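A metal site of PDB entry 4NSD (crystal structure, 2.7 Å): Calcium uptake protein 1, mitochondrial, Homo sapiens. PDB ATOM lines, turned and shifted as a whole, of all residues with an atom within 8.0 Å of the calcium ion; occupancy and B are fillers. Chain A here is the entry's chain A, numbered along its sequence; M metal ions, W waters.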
ATOM      1  N   PHE A 134     -15.023  -3.237 -18.819  1.00  0.00           N
ATOM      2  CA  PHE A 134     -15.717  -2.120 -19.462  1.00  0.00           C
ATOM      3  C   PHE A 134     -17.137  -2.053 -18.945  1.00  0.00           C
ATOM      4  O   PHE A 134     -17.663  -0.986 -18.654  1.00  0.00           O
ATOM      5  CB  PHE A 134     -15.721  -2.308 -20.979  1.00  0.00           C
ATOM      6  CG  PHE A 134     -16.320  -1.139 -21.726  1.00  0.00           C
ATOM      7  CD1 PHE A 134     -15.509  -0.170 -22.294  1.00  0.00           C
ATOM      8  CD2 PHE A 134     -17.686  -1.004 -21.827  1.00  0.00           C
ATOM      9  CE1 PHE A 134     -16.045   0.893 -22.957  1.00  0.00           C
ATOM     10  CE2 PHE A 134     -18.235   0.070 -22.488  1.00  0.00           C
ATOM     11  CZ  PHE A 134     -17.412   1.018 -23.057  1.00  0.00           C
ATOM     12  N   LYS A 135     -17.771  -3.221 -18.871  1.00  0.00           N
ATOM     13  CA  LYS A 135     -19.091  -3.376 -18.287  1.00  0.00           C
ATOM     14  C   LYS A 135     -19.158  -2.676 -16.937  1.00  0.00           C
ATOM     15  O   LYS A 135     -19.890  -1.709 -16.768  1.00  0.00           O
ATOM     16  CB  LYS A 135     -19.379  -4.864 -18.063  1.00  0.00           C
ATOM     17  CG  LYS A 135     -20.322  -5.504 -19.058  1.00  0.00           C
ATOM     18  CD  LYS A 135     -20.426  -7.007 -18.768  1.00  0.00           C
ATOM     19  CE  LYS A 135     -21.696  -7.630 -19.366  1.00  0.00           C
ATOM     20  NZ  LYS A 135     -22.975  -7.194 -18.703  1.00  0.00           N
ATOM     21  N   PHE A 137     -17.379  -0.668 -15.438  1.00  0.00           N
ATOM     22  CA  PHE A 137     -17.085   0.758 -15.491  1.00  0.00           C
ATOM     23  C   PHE A 137     -18.234   1.568 -16.100  1.00  0.00           C
ATOM     24  O   PHE A 137     -18.608   2.611 -15.569  1.00  0.00           O
ATOM     25  CB  PHE A 137     -15.779   1.027 -16.235  1.00  0.00           C
ATOM     26  CG  PHE A 137     -14.574   1.022 -15.339  1.00  0.00           C
ATOM     27  CD1 PHE A 137     -13.835  -0.129 -15.157  1.00  0.00           C
ATOM     28  CD2 PHE A 137     -14.197   2.170 -14.671  1.00  0.00           C
ATOM     29  CE1 PHE A 137     -12.738  -0.134 -14.333  1.00  0.00           C
ATOM     30  CE2 PHE A 137     -13.097   2.175 -13.834  1.00  0.00           C
ATOM     31  CZ  PHE A 137     -12.360   1.023 -13.667  1.00  0.00           C
ATOM     32  N   ASP A 138     -18.769   1.100 -17.200  1.00  0.00           N
ATOM     33  CA  ASP A 138     -19.910   1.734 -17.838  1.00  0.00           C
ATOM     34  C   ASP A 138     -21.114   1.720 -16.907  1.00  0.00           C
ATOM     35  O   ASP A 138     -21.945   0.805 -16.956  1.00  0.00           O
ATOM     36  CB  ASP A 138     -20.247   0.979 -19.124  1.00  0.00           C
ATOM     37  CG  ASP A 138     -21.424   1.566 -19.851  1.00  0.00           C
ATOM     38  OD1 ASP A 138     -21.736   2.756 -19.592  1.00  0.00           O
ATOM     39  OD2 ASP A 138     -22.025   0.831 -20.673  1.00  0.00           O
ATOM     40  N   LEU A 139     -21.213   2.749 -16.067  1.00  0.00           N
ATOM     41  CA  LEU A 139     -22.196   2.777 -14.982  1.00  0.00           C
ATOM     42  C   LEU A 139     -23.627   2.976 -15.453  1.00  0.00           C
ATOM     43  O   LEU A 139     -24.544   2.307 -14.980  1.00  0.00           O
ATOM     44  CB  LEU A 139     -21.838   3.844 -13.962  1.00  0.00           C
ATOM     45  CG  LEU A 139     -20.702   3.456 -13.014  1.00  0.00           C
ATOM     46  CD1 LEU A 139     -19.985   4.674 -12.494  1.00  0.00           C
ATOM     47  CD2 LEU A 139     -21.239   2.612 -11.869  1.00  0.00           C
ATOM     48  N   ASN A 140     -23.823   3.885 -16.386  1.00  0.00           N
ATOM     49  CA  ASN A 140     -25.158   4.104 -16.893  1.00  0.00           C
ATOM     50  C   ASN A 140     -25.444   3.139 -18.039  1.00  0.00           C
ATOM     51  O   ASN A 140     -26.465   3.257 -18.708  1.00  0.00           O
ATOM     52  CB  ASN A 140     -25.338   5.548 -17.353  1.00  0.00           C
ATOM     53  CG  ASN A 140     -24.325   5.926 -18.396  1.00  0.00           C
ATOM     54  OD1 ASN A 140     -23.625   5.060 -18.931  1.00  0.00           O
ATOM     55  ND2 ASN A 140     -24.253   7.217 -18.710  1.00  0.00           N
ATOM     56  N   GLY A 141     -24.538   2.194 -18.252  1.00  0.00           N
ATOM     57  CA  GLY A 141     -24.667   1.245 -19.343  1.00  0.00           C
ATOM     58  C   GLY A 141     -24.969   1.873 -20.691  1.00  0.00           C
ATOM     59  O   GLY A 141     -25.711   1.310 -21.502  1.00  0.00           O
ATOM     60  N   ASP A 142     -24.399   3.054 -20.957  1.00  0.00           N
ATOM     61  CA  ASP A 142     -24.707   3.765 -22.188  1.00  0.00           C
ATOM     62  C   ASP A 142     -23.708   3.449 -23.314  1.00  0.00           C
ATOM     63  O   ASP A 142     -23.482   4.283 -24.194  1.00  0.00           O
ATOM     64  CB  ASP A 142     -24.746   5.268 -21.943  1.00  0.00           C
ATOM     65  CG  ASP A 142     -23.348   5.843 -21.786  1.00  0.00           C
ATOM     66  OD1 ASP A 142     -22.425   5.019 -21.630  1.00  0.00           O
ATOM     67  OD2 ASP A 142     -23.178   7.087 -21.832  1.00  0.00           O
ATOM     68  N   GLY A 143     -23.107   2.262 -23.268  1.00  0.00           N
ATOM     69  CA  GLY A 143     -22.148   1.820 -24.280  1.00  0.00           C
ATOM     70  C   GLY A 143     -20.804   2.551 -24.294  1.00  0.00           C
ATOM     71  O   GLY A 143     -19.868   2.146 -24.986  1.00  0.00           O
ATOM     72  N   GLU A 144     -20.721   3.637 -23.547  1.00  0.00           N
ATOM     73  CA  GLU A 144     -19.482   4.399 -23.442  1.00  0.00           C
ATOM     74  C   GLU A 144     -18.931   4.325 -22.038  1.00  0.00           C
ATOM     75  O   GLU A 144     -19.484   3.663 -21.175  1.00  0.00           O
ATOM     76  CB  GLU A 144     -19.736   5.863 -23.772  1.00  0.00           C
ATOM     77  CG  GLU A 144     -19.950   6.147 -25.249  1.00  0.00           C
ATOM     78  CD  GLU A 144     -20.118   7.622 -25.511  1.00  0.00           C
ATOM     79  OE1 GLU A 144     -20.666   8.314 -24.628  1.00  0.00           O
ATOM     80  OE2 GLU A 144     -19.696   8.098 -26.591  1.00  0.00           O
ATOM     81  N   VAL A 145     -17.804   4.994 -21.836  1.00  0.00           N
ATOM     82  CA  VAL A 145     -17.179   5.137 -20.527  1.00  0.00           C
ATOM     83  C   VAL A 145     -16.418   6.447 -20.502  1.00  0.00           C
ATOM     84  O   VAL A 145     -15.650   6.754 -21.432  1.00  0.00           O
ATOM     85  CB  VAL A 145     -16.166   4.027 -20.252  1.00  0.00           C
ATOM     86  CG1 VAL A 145     -15.387   4.374 -18.993  1.00  0.00           C
ATOM     87  CG2 VAL A 145     -16.847   2.675 -20.144  1.00  0.00           C
ATOM     88  N   ASP A 146     -16.629   7.226 -19.442  1.00  0.00           N
ATOM     89  CA  ASP A 146     -16.074   8.575 -19.380  1.00  0.00           C
ATOM     90  C   ASP A 146     -15.211   8.845 -18.137  1.00  0.00           C
ATOM     91  O   ASP A 146     -14.963   7.950 -17.318  1.00  0.00           O
ATOM     92  CB  ASP A 146     -17.191   9.611 -19.481  1.00  0.00           C
ATOM     93  CG  ASP A 146     -18.382   9.302 -18.568  1.00  0.00           C
ATOM     94  OD1 ASP A 146     -18.226   9.358 -17.329  1.00  0.00           O
ATOM     95  OD2 ASP A 146     -19.466   9.006 -19.104  1.00  0.00           O
ATOM     96  N   GLU A 149     -17.373   8.755 -14.776  1.00  0.00           N
ATOM     97  CA  GLU A 149     -17.606   7.373 -14.385  1.00  0.00           C
ATOM     98  C   GLU A 149     -16.355   6.700 -13.838  1.00  0.00           C
ATOM     99  O   GLU A 149     -16.386   6.096 -12.766  1.00  0.00           O
ATOM    100  CB  GLU A 149     -18.156   6.566 -15.551  1.00  0.00           C
ATOM    101  CG  GLU A 149     -19.650   6.356 -15.477  1.00  0.00           C
ATOM    102  CD  GLU A 149     -20.234   6.006 -16.812  1.00  0.00           C
ATOM    103  OE1 GLU A 149     -19.465   6.045 -17.795  1.00  0.00           O
ATOM    104  OE2 GLU A 149     -21.444   5.701 -16.873  1.00  0.00           O
ATOM    105  N   PHE A 150     -15.253   6.792 -14.582  1.00  0.00           N
ATOM    106  CA  PHE A 150     -13.997   6.290 -14.046  1.00  0.00           C
ATOM    107  C   PHE A 150     -13.800   6.913 -12.676  1.00  0.00           C
ATOM    108  O   PHE A 150     -13.508   6.225 -11.690  1.00  0.00           O
ATOM    109  CB  PHE A 150     -12.818   6.630 -14.960  1.00  0.00           C
ATOM    110  CG  PHE A 150     -11.525   6.004 -14.514  1.00  0.00           C
ATOM    111  CD1 PHE A 150     -10.900   5.056 -15.293  1.00  0.00           C
ATOM    112  CD2 PHE A 150     -10.957   6.351 -13.300  1.00  0.00           C
ATOM    113  CE1 PHE A 150      -9.718   4.475 -14.879  1.00  0.00           C
ATOM    114  CE2 PHE A 150      -9.780   5.771 -12.878  1.00  0.00           C
ATOM    115  CZ  PHE A 150      -9.158   4.832 -13.672  1.00  0.00           C
ATOM    116  N   LYS A 197     -14.472   9.605 -24.531  1.00  0.00           N
ATOM    117  CA  LYS A 197     -15.307   8.470 -24.196  1.00  0.00           C
ATOM    118  C   LYS A 197     -14.793   7.184 -24.826  1.00  0.00           C
ATOM    119  O   LYS A 197     -14.606   7.106 -26.037  1.00  0.00           O
ATOM    120  CB  LYS A 197     -16.756   8.738 -24.605  1.00  0.00           C
ATOM    121  CG  LYS A 197     -17.456   9.772 -23.732  1.00  0.00           C
ATOM    122  CD  LYS A 197     -18.725  10.283 -24.375  1.00  0.00           C
ATOM    123  CE  LYS A 197     -18.446  10.898 -25.744  1.00  0.00           C
ATOM    124  NZ  LYS A 197     -17.579  12.109 -25.645  1.00  0.00           N
ATOM    125  N   LEU A 198     -14.600   6.185 -23.978  1.00  0.00           N
ATOM    126  CA  LEU A 198     -13.944   4.939 -24.336  1.00  0.00           C
ATOM    127  C   LEU A 198     -14.954   3.874 -24.762  1.00  0.00           C
ATOM    128  O   LEU A 198     -15.961   3.664 -24.105  1.00  0.00           O
ATOM    129  CB  LEU A 198     -13.156   4.445 -23.120  1.00  0.00           C
ATOM    130  CG  LEU A 198     -12.067   3.382 -23.191  1.00  0.00           C
ATOM    131  CD1 LEU A 198     -12.090   2.549 -21.896  1.00  0.00           C
ATOM    132  CD2 LEU A 198     -12.202   2.498 -24.419  1.00  0.00           C
HETATM  133 CA    CA M   1     -21.074   5.161 -19.589  1.00  0.00          CA
HETATM  134  O   HOH W   1     -21.328   7.679 -19.964  1.00  0.00           O
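The side-chain carboxylate (OD1) of Asp 146 lies within hydrogen-bond range of the backbone NH (N) of Glu 149.
The backbone NH (N) of Gly 141 lies close to the side-chain carboxylate (OD1) of Asp 138 (3.2 Å).
The backbone NH of Leu 139 lies close to the side-chain carboxylate of Glu 149, 3.1 Å away.
The backbone NH (N) of Gly 143 sits at hydrogen-bond distance from the side-chain carboxylate (OD2) of Asp 138 (3.2 Å).
The backbone carbonyl oxygen of Val 145 lies within hydrogen-bond range of the backbone NH of Leu 198 (2.8 Å).
Residues that only touch the calcium ion: Val 145 (3.97 Å).
Six residues have an atom within 4 Å of the calcium ion: Asp 138, Asn 140, Asp 142, Glu 144, Val 145 and Glu 149.
The nearest printed residue that does not touch the calcium ion is Asp 146 (4.2 Å).
The calcium ion is bound by the side-chain carboxylate (OD1) of Asp 142, the side-chain carboxylate (OD1) of Asp 138, water W1, the side-chain carboxylate (OE1) of Glu 149, the side-chain amide oxygen (OD1) of Asn 140, the backbone carbonyl oxygen (O) of Glu 144 and the side-chain carboxylate (OE2) of Glu 149.
Water W1 lies within hydrogen-bond range of OD2 of Asp 146 (2.4 Å), OD2 of Asp 142 (2.7 Å) and ND2 of Asn 140 (3.2 Å).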
